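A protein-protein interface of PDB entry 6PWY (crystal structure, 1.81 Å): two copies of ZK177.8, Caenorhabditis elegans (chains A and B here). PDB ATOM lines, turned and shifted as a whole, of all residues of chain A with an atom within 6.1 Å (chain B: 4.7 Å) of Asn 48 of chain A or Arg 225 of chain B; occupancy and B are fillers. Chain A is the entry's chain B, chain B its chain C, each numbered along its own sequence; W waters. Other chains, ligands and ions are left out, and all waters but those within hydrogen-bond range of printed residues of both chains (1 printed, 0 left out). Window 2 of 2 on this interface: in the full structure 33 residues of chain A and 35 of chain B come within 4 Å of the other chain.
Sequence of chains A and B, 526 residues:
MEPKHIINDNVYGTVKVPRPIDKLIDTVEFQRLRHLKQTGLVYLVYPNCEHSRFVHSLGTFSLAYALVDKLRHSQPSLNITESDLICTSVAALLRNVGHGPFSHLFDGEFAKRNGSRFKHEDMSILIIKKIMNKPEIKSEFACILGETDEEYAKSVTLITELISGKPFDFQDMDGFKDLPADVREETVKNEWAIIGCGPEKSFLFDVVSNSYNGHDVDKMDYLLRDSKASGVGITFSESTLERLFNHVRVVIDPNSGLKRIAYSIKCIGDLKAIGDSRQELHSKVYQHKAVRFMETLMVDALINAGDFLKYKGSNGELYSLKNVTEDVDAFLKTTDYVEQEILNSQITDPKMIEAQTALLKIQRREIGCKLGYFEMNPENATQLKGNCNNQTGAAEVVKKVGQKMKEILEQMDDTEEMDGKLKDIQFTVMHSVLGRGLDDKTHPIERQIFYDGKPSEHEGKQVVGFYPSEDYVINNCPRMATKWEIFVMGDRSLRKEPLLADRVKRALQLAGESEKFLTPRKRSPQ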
ATOM      1  N   TYR A  43       2.301   9.125 -36.676  1.00  0.00           N
ATOM      2  CA  TYR A  43       3.054   8.549 -35.543  1.00  0.00           C
ATOM      3  C   TYR A  43       3.936   9.595 -34.843  1.00  0.00           C
ATOM      4  O   TYR A  43       4.301   9.387 -33.694  1.00  0.00           O
ATOM      5  CB  TYR A  43       3.877   7.328 -35.978  1.00  0.00           C
ATOM      6  CG  TYR A  43       5.158   7.624 -36.716  1.00  0.00           C
ATOM      7  CD1 TYR A  43       5.195   8.430 -37.826  1.00  0.00           C
ATOM      8  CD2 TYR A  43       6.336   6.970 -36.374  1.00  0.00           C
ATOM      9  CE1 TYR A  43       6.365   8.629 -38.544  1.00  0.00           C
ATOM     10  CE2 TYR A  43       7.519   7.151 -37.074  1.00  0.00           C
ATOM     11  CZ  TYR A  43       7.538   8.043 -38.115  1.00  0.00           C
ATOM     12  OH  TYR A  43       8.662   8.199 -38.842  1.00  0.00           O
ATOM     13  N   TYR A  46       1.018  10.642 -32.430  1.00  0.00           N
ATOM     14  CA  TYR A  46       0.403   9.451 -31.831  1.00  0.00           C
ATOM     15  C   TYR A  46       1.363   8.288 -32.055  1.00  0.00           C
ATOM     16  O   TYR A  46       1.289   7.597 -33.078  1.00  0.00           O
ATOM     17  CB  TYR A  46      -0.947   9.157 -32.488  1.00  0.00           C
ATOM     18  CG  TYR A  46      -2.048  10.157 -32.261  1.00  0.00           C
ATOM     19  CD1 TYR A  46      -2.222  11.221 -33.112  1.00  0.00           C
ATOM     20  CD2 TYR A  46      -2.999   9.953 -31.273  1.00  0.00           C
ATOM     21  CE1 TYR A  46      -3.292  12.082 -32.998  1.00  0.00           C
ATOM     22  CE2 TYR A  46      -4.095  10.762 -31.173  1.00  0.00           C
ATOM     23  CZ  TYR A  46      -4.226  11.861 -32.011  1.00  0.00           C
ATOM     24  OH  TYR A  46      -5.303  12.666 -31.878  1.00  0.00           O
ATOM     25  N   PRO A  47       2.376   8.087 -31.176  1.00  0.00           N
ATOM     26  CA  PRO A  47       3.454   7.142 -31.481  1.00  0.00           C
ATOM     27  C   PRO A  47       3.055   5.695 -31.659  1.00  0.00           C
ATOM     28  O   PRO A  47       3.778   4.961 -32.279  1.00  0.00           O
ATOM     29  CB  PRO A  47       4.421   7.292 -30.305  1.00  0.00           C
ATOM     30  CG  PRO A  47       4.151   8.674 -29.802  1.00  0.00           C
ATOM     31  CD  PRO A  47       2.643   8.821 -29.958  1.00  0.00           C
ATOM     32  N   ASN A  48       1.874   5.334 -31.166  1.00  0.00           N
ATOM     33  CA  ASN A  48       1.305   3.978 -31.342  1.00  0.00           C
ATOM     34  C   ASN A  48       0.692   3.798 -32.734  1.00  0.00           C
ATOM     35  O   ASN A  48       0.405   2.673 -33.110  1.00  0.00           O
ATOM     36  CB  ASN A  48       0.372   3.682 -30.168  1.00  0.00           C
ATOM     37  CG  ASN A  48       1.047   2.673 -29.242  1.00  0.00           C
ATOM     38  OD1 ASN A  48       0.813   1.471 -29.450  1.00  0.00           O
ATOM     39  ND2 ASN A  48       1.887   3.080 -28.269  1.00  0.00           N
ATOM     40  N   CYS A  49       0.474   4.846 -33.514  1.00  0.00           N
ATOM     41  CA  CYS A  49       0.022   4.744 -34.923  1.00  0.00           C
ATOM     42  C   CYS A  49       1.146   4.365 -35.838  1.00  0.00           C
ATOM     43  O   CYS A  49       1.397   5.109 -36.807  1.00  0.00           O
ATOM     44  CB  CYS A  49      -0.566   5.994 -35.491  1.00  0.00           C
ATOM     45  SG  CYS A  49      -2.214   6.266 -34.789  1.00  0.00           S
ATOM     46  N   GLU A  50       1.763   3.200 -35.564  1.00  0.00           N
ATOM     47  CA  GLU A  50       2.869   2.712 -36.402  1.00  0.00           C
ATOM     48  C   GLU A  50       2.411   1.434 -37.079  1.00  0.00           C
ATOM     49  O   GLU A  50       3.258   0.662 -37.539  1.00  0.00           O
ATOM     50  CB  GLU A  50       4.177   2.707 -35.577  1.00  0.00           C
ATOM     51  CG  GLU A  50       4.036   2.117 -34.214  1.00  0.00           C
ATOM     52  CD  GLU A  50       5.269   2.107 -33.258  1.00  0.00           C
ATOM     53  OE1 GLU A  50       6.325   2.790 -33.528  1.00  0.00           O
ATOM     54  OE2 GLU A  50       5.125   1.461 -32.215  1.00  0.00           O
ATOM     55  N   HIS A  51       1.103   1.219 -37.183  1.00  0.00           N
ATOM     56  CA  HIS A  51       0.540   0.031 -37.854  1.00  0.00           C
ATOM     57  C   HIS A  51       0.752   0.190 -39.362  1.00  0.00           C
ATOM     58  O   HIS A  51       0.700   1.315 -39.882  1.00  0.00           O
ATOM     59  CB  HIS A  51      -0.917  -0.209 -37.481  1.00  0.00           C
ATOM     60  CG  HIS A  51      -1.850   0.946 -37.716  1.00  0.00           C
ATOM     61  ND1 HIS A  51      -1.699   2.164 -37.090  1.00  0.00           N
ATOM     62  CD2 HIS A  51      -2.919   1.066 -38.519  1.00  0.00           C
ATOM     63  CE1 HIS A  51      -2.688   2.987 -37.492  1.00  0.00           C
ATOM     64  NE2 HIS A  51      -3.449   2.320 -38.350  1.00  0.00           N
ATOM     65  N   ALA A 229      -5.460   2.304 -32.601  1.00  0.00           N
ATOM     66  CA  ALA A 229      -4.018   2.653 -32.599  1.00  0.00           C
ATOM     67  C   ALA A 229      -3.823   4.052 -32.013  1.00  0.00           C
ATOM     68  O   ALA A 229      -2.806   4.249 -31.340  1.00  0.00           O
ATOM     69  CB  ALA A 229      -3.477   2.621 -34.016  1.00  0.00           C
ATOM     70  N   SER A 230      -4.723   5.001 -32.283  1.00  0.00           N
ATOM     71  CA  SER A 230      -4.626   6.407 -31.856  1.00  0.00           C
ATOM     72  C   SER A 230      -5.077   6.552 -30.408  1.00  0.00           C
ATOM     73  O   SER A 230      -4.664   7.563 -29.784  1.00  0.00           O
ATOM     74  CB  SER A 230      -5.439   7.307 -32.772  1.00  0.00           C
ATOM     75  OG  SER A 230      -6.844   7.016 -32.656  1.00  0.00           O
ATOM     76  N   ASP B   9      -0.480   6.568 -25.099  1.00  0.00           N
ATOM     77  CA  ASP B   9       0.224   5.262 -25.002  1.00  0.00           C
ATOM     78  C   ASP B   9      -0.870   4.200 -24.858  1.00  0.00           C
ATOM     79  O   ASP B   9      -1.735   4.368 -24.003  1.00  0.00           O
ATOM     80  CB  ASP B   9       1.237   5.290 -23.851  1.00  0.00           C
ATOM     81  CG  ASP B   9       1.883   3.942 -23.493  1.00  0.00           C
ATOM     82  OD1 ASP B   9       1.171   2.977 -23.077  1.00  0.00           O
ATOM     83  OD2 ASP B   9       3.120   3.871 -23.598  1.00  0.00           O
ATOM     84  N   ASN B  10      -0.763   3.118 -25.582  1.00  0.00           N
ATOM     85  CA  ASN B  10      -1.868   2.108 -25.635  1.00  0.00           C
ATOM     86  C   ASN B  10      -1.837   1.252 -24.371  1.00  0.00           C
ATOM     87  O   ASN B  10      -2.814   0.640 -24.114  1.00  0.00           O
ATOM     88  CB  ASN B  10      -1.829   1.294 -26.940  1.00  0.00           C
ATOM     89  CG  ASN B  10      -0.612   0.389 -27.019  1.00  0.00           C
ATOM     90  OD1 ASN B  10       0.493   0.767 -26.685  1.00  0.00           O
ATOM     91  ND2 ASN B  10      -0.816  -0.917 -27.247  1.00  0.00           N
ATOM     92  N   VAL B  11      -0.735   1.195 -23.631  1.00  0.00           N
ATOM     93  CA  VAL B  11      -0.645   0.362 -22.388  1.00  0.00           C
ATOM     94  C   VAL B  11      -1.179   1.142 -21.185  1.00  0.00           C
ATOM     95  O   VAL B  11      -2.040   0.585 -20.474  1.00  0.00           O
ATOM     96  CB  VAL B  11       0.773  -0.148 -22.127  1.00  0.00           C
ATOM     97  CG1 VAL B  11       0.851  -0.945 -20.838  1.00  0.00           C
ATOM     98  CG2 VAL B  11       1.295  -0.962 -23.300  1.00  0.00           C
ATOM     99  N   TYR B  12      -0.796   2.400 -21.006  1.00  0.00           N
ATOM    100  CA  TYR B  12      -1.118   3.199 -19.799  1.00  0.00           C
ATOM    101  C   TYR B  12      -2.179   4.261 -20.103  1.00  0.00           C
ATOM    102  O   TYR B  12      -2.505   4.972 -19.159  1.00  0.00           O
ATOM    103  CB  TYR B  12       0.154   3.867 -19.262  1.00  0.00           C
ATOM    104  CG  TYR B  12       1.281   2.880 -19.098  1.00  0.00           C
ATOM    105  CD1 TYR B  12       1.180   1.823 -18.182  1.00  0.00           C
ATOM    106  CD2 TYR B  12       2.436   3.002 -19.852  1.00  0.00           C
ATOM    107  CE1 TYR B  12       2.193   0.892 -18.056  1.00  0.00           C
ATOM    108  CE2 TYR B  12       3.452   2.065 -19.738  1.00  0.00           C
ATOM    109  CZ  TYR B  12       3.321   1.004 -18.847  1.00  0.00           C
ATOM    110  OH  TYR B  12       4.311   0.071 -18.800  1.00  0.00           O
ATOM    111  N   HIS B  51       5.579  -2.725 -32.986  1.00  0.00           N
ATOM    112  CA  HIS B  51       5.784  -1.593 -32.057  1.00  0.00           C
ATOM    113  C   HIS B  51       7.301  -1.346 -31.991  1.00  0.00           C
ATOM    114  O   HIS B  51       8.096  -2.288 -32.118  1.00  0.00           O
ATOM    115  CB  HIS B  51       5.169  -1.861 -30.684  1.00  0.00           C
ATOM    116  CG  HIS B  51       5.597  -3.134 -30.025  1.00  0.00           C
ATOM    117  ND1 HIS B  51       5.355  -4.384 -30.564  1.00  0.00           N
ATOM    118  CD2 HIS B  51       6.239  -3.359 -28.867  1.00  0.00           C
ATOM    119  CE1 HIS B  51       5.821  -5.334 -29.726  1.00  0.00           C
ATOM    120  NE2 HIS B  51       6.351  -4.711 -28.677  1.00  0.00           N
ATOM    121  N   VAL B  55       8.417   3.500 -28.328  1.00  0.00           N
ATOM    122  CA  VAL B  55       7.253   3.412 -27.430  1.00  0.00           C
ATOM    123  C   VAL B  55       7.631   2.651 -26.177  1.00  0.00           C
ATOM    124  O   VAL B  55       7.177   3.069 -25.064  1.00  0.00           O
ATOM    125  CB  VAL B  55       5.959   2.938 -28.083  1.00  0.00           C
ATOM    126  CG1 VAL B  55       5.576   3.877 -29.239  1.00  0.00           C
ATOM    127  CG2 VAL B  55       6.014   1.524 -28.639  1.00  0.00           C
ATOM    128  N   HIS B  56       8.394   1.584 -26.278  1.00  0.00           N
ATOM    129  CA  HIS B  56       8.860   0.872 -25.067  1.00  0.00           C
ATOM    130  C   HIS B  56       9.675   1.813 -24.157  1.00  0.00           C
ATOM    131  O   HIS B  56       9.511   1.774 -22.879  1.00  0.00           O
ATOM    132  CB  HIS B  56       9.582  -0.424 -25.421  1.00  0.00           C
ATOM    133  CG  HIS B  56      10.301  -1.030 -24.259  1.00  0.00           C
ATOM    134  ND1 HIS B  56       9.626  -1.472 -23.122  1.00  0.00           N
ATOM    135  CD2 HIS B  56      11.615  -1.226 -24.028  1.00  0.00           C
ATOM    136  CE1 HIS B  56      10.548  -1.980 -22.278  1.00  0.00           C
ATOM    137  NE2 HIS B  56      11.743  -1.779 -22.762  1.00  0.00           N
ATOM    138  N   GLY B  59       7.496   4.247 -22.236  1.00  0.00           N
ATOM    139  CA  GLY B  59       6.750   3.541 -21.201  1.00  0.00           C
ATOM    140  C   GLY B  59       7.614   3.235 -19.998  1.00  0.00           C
ATOM    141  O   GLY B  59       7.162   3.419 -18.865  1.00  0.00           O
ATOM    142  N   ASP B 221       7.308  -3.144 -18.283  1.00  0.00           N
ATOM    143  CA  ASP B 221       6.751  -2.484 -19.480  1.00  0.00           C
ATOM    144  C   ASP B 221       6.702  -3.489 -20.634  1.00  0.00           C
ATOM    145  O   ASP B 221       5.677  -3.549 -21.289  1.00  0.00           O
ATOM    146  CB  ASP B 221       7.513  -1.250 -19.930  1.00  0.00           C
ATOM    147  CG  ASP B 221       6.838  -0.610 -21.157  1.00  0.00           C
ATOM    148  OD1 ASP B 221       5.908   0.205 -20.926  1.00  0.00           O
ATOM    149  OD2 ASP B 221       7.191  -0.989 -22.332  1.00  0.00           O
ATOM    150  N   TYR B 222       7.768  -4.242 -20.926  1.00  0.00           N
ATOM    151  CA  TYR B 222       7.793  -5.052 -22.162  1.00  0.00           C
ATOM    152  C   TYR B 222       6.822  -6.236 -22.011  1.00  0.00           C
ATOM    153  O   TYR B 222       6.182  -6.595 -23.011  1.00  0.00           O
ATOM    154  CB  TYR B 222       9.195  -5.420 -22.580  1.00  0.00           C
ATOM    155  CG  TYR B 222       9.902  -6.625 -22.003  1.00  0.00           C
ATOM    156  CD1 TYR B 222       9.382  -7.895 -22.184  1.00  0.00           C
ATOM    157  CD2 TYR B 222      11.110  -6.514 -21.373  1.00  0.00           C
ATOM    158  CE1 TYR B 222      10.060  -9.006 -21.719  1.00  0.00           C
ATOM    159  CE2 TYR B 222      11.788  -7.604 -20.908  1.00  0.00           C
ATOM    160  CZ  TYR B 222      11.264  -8.858 -21.090  1.00  0.00           C
ATOM    161  OH  TYR B 222      11.902  -9.999 -20.685  1.00  0.00           O
ATOM    162  N   LEU B 223       6.638  -6.769 -20.818  1.00  0.00           N
ATOM    163  CA  LEU B 223       5.662  -7.866 -20.652  1.00  0.00           C
ATOM    164  C   LEU B 223       4.287  -7.330 -21.003  1.00  0.00           C
ATOM    165  O   LEU B 223       3.538  -8.040 -21.779  1.00  0.00           O
ATOM    166  CB  LEU B 223       5.701  -8.424 -19.224  1.00  0.00           C
ATOM    167  CG  LEU B 223       6.951  -9.169 -18.804  1.00  0.00           C
ATOM    168  CD1 LEU B 223       6.799  -9.495 -17.322  1.00  0.00           C
ATOM    169  CD2 LEU B 223       7.158 -10.421 -19.628  1.00  0.00           C
ATOM    170  N   LEU B 224       3.885  -6.181 -20.454  1.00  0.00           N
ATOM    171  CA  LEU B 224       2.553  -5.664 -20.780  1.00  0.00           C
ATOM    172  C   LEU B 224       2.441  -5.345 -22.268  1.00  0.00           C
ATOM    173  O   LEU B 224       1.382  -5.610 -22.872  1.00  0.00           O
ATOM    174  CB  LEU B 224       2.302  -4.401 -19.942  1.00  0.00           C
ATOM    175  CG  LEU B 224       2.207  -4.652 -18.449  1.00  0.00           C
ATOM    176  CD1 LEU B 224       1.966  -3.351 -17.780  1.00  0.00           C
ATOM    177  CD2 LEU B 224       1.105  -5.651 -18.101  1.00  0.00           C
ATOM    178  N   ARG B 225       3.439  -4.652 -22.803  1.00  0.00           N
ATOM    179  CA  ARG B 225       3.380  -4.121 -24.185  1.00  0.00           C
ATOM    180  C   ARG B 225       3.423  -5.289 -25.179  1.00  0.00           C
ATOM    181  O   ARG B 225       2.698  -5.266 -26.196  1.00  0.00           O
ATOM    182  CB  ARG B 225       4.499  -3.102 -24.407  1.00  0.00           C
ATOM    183  CG  ARG B 225       4.401  -2.290 -25.698  1.00  0.00           C
ATOM    184  CD  ARG B 225       5.493  -1.170 -25.729  1.00  0.00           C
ATOM    185  NE  ARG B 225       5.370  -0.333 -24.544  1.00  0.00           N
ATOM    186  CZ  ARG B 225       4.511   0.694 -24.403  1.00  0.00           C
ATOM    187  NH1 ARG B 225       3.733   1.057 -25.417  1.00  0.00           N
ATOM    188  NH2 ARG B 225       4.450   1.341 -23.250  1.00  0.00           N
ATOM    189  N   ASP B 226       4.285  -6.256 -24.965  1.00  0.00           N
ATOM    190  CA  ASP B 226       4.525  -7.375 -25.919  1.00  0.00           C
ATOM    191  C   ASP B 226       3.332  -8.357 -25.840  1.00  0.00           C
ATOM    192  O   ASP B 226       2.946  -8.821 -26.892  1.00  0.00           O
ATOM    193  CB  ASP B 226       5.821  -8.124 -25.641  1.00  0.00           C
ATOM    194  CG  ASP B 226       7.098  -7.278 -25.826  1.00  0.00           C
ATOM    195  OD1 ASP B 226       7.000  -6.113 -26.318  1.00  0.00           O
ATOM    196  OD2 ASP B 226       8.211  -7.845 -25.516  1.00  0.00           O
ATOM    197  N   SER B 227       2.728  -8.516 -24.661  1.00  0.00           N
ATOM    198  CA  SER B 227       1.492  -9.303 -24.519  1.00  0.00           C
ATOM    199  C   SER B 227       0.372  -8.634 -25.347  1.00  0.00           C
ATOM    200  O   SER B 227      -0.372  -9.333 -26.055  1.00  0.00           O
ATOM    201  CB  SER B 227       1.068  -9.414 -23.054  1.00  0.00           C
ATOM    202  OG  SER B 227      -0.290  -9.940 -23.016  1.00  0.00           O
ATOM    203  N   LYS B 228       0.196  -7.334 -25.199  1.00  0.00           N
ATOM    204  CA  LYS B 228      -0.899  -6.644 -25.920  1.00  0.00           C
ATOM    205  C   LYS B 228      -0.629  -6.708 -27.425  1.00  0.00           C
ATOM    206  O   LYS B 228      -1.563  -6.916 -28.187  1.00  0.00           O
ATOM    207  CB  LYS B 228      -0.969  -5.206 -25.429  1.00  0.00           C
ATOM    208  CG  LYS B 228      -2.326  -4.556 -25.593  1.00  0.00           C
ATOM    209  CD  LYS B 228      -2.391  -3.254 -24.756  1.00  0.00           C
ATOM    210  CE  LYS B 228      -3.294  -2.241 -25.415  1.00  0.00           C
ATOM    211  NZ  LYS B 228      -4.648  -2.779 -25.376  1.00  0.00           N
ATOM    212  N   ALA B 229       0.596  -6.490 -27.863  1.00  0.00           N
ATOM    213  CA  ALA B 229       0.889  -6.453 -29.322  1.00  0.00           C
ATOM    214  C   ALA B 229       0.733  -7.855 -29.945  1.00  0.00           C
ATOM    215  O   ALA B 229       0.271  -7.932 -31.095  1.00  0.00           O
ATOM    216  CB  ALA B 229       2.312  -5.941 -29.537  1.00  0.00           C
HETATM  217  O   HOH W   1       2.721  -0.411 -27.796  1.00  0.00           O
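The side-chain amide oxygen (OD1) of Asn 10 of chain B sits close to the side-chain amide oxygen (OD1) of Asn 48 of chain A (2.9 Å).
Among the printed residues, merely in contact across the chains: Glu 50 of chain A with His 51 of chain B, Glu 50 of chain A with Val 55 of chain B, Pro 47 of chain A with Val 55 of chain B, Asn 48 of chain A with Val 55 of chain B and Asn 48 of chain A with Arg 225 of chain B.
The side-chain amide oxygen of Asn 10 of chain B lies within hydrogen-bond range of the guanidinium group of Arg 225 of chain B.
NE2 of His 51 of chain B lies within hydrogen-bond range of OD1 of Asp 226 of chain B.
NE of Arg 225 of chain B lies within salt-bridge range of OD2 of Asp 221 of chain B.
The side-chain carboxylate (OD2) of Asp 9 of chain B is in salt-bridge range of the guanidinium group (NH2) of Arg 225 of chain B (2.9 Å).
Water W1 lies within hydrogen-bond range of the side-chain amide oxygen (OD1) of Asn 10 of chain B (2.8 Å), the guanidinium group (NH1) of Arg 225 of chain B (3.0 Å) and the side-chain amide oxygen (OD1) of Asn 48 of chain A (3.1 Å).
Positions printed for both chains: 51 and 229.
Of the 6 pairs that touch across the chains among the printed residues, none has its exchanged pair printed and touching as well.
Asn 48 of chain A touches three residues of chain B.
His 51 of chain A touches none of the printed residues of chain B.
Printed residues of chain A within 4 Å of Asn 10 of chain B: Asn 48 (2.9 Å).
Of the printed residues of chain A, Val 55 of chain B touches Pro 47, Asn 48 and Glu 50.
Arg 225 of chain B touches just one residue of chain A: Asn 48 (3.95 Å).
Asp 226 of chain B touches none of the printed residues of chain A.
The nearest residue of chain B that does not touch Asn 48 of chain A is Asp 9 of chain B (4.3 Å).
Of the 9 printed residues of chain A, 3 touch a printed residue of chain B.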
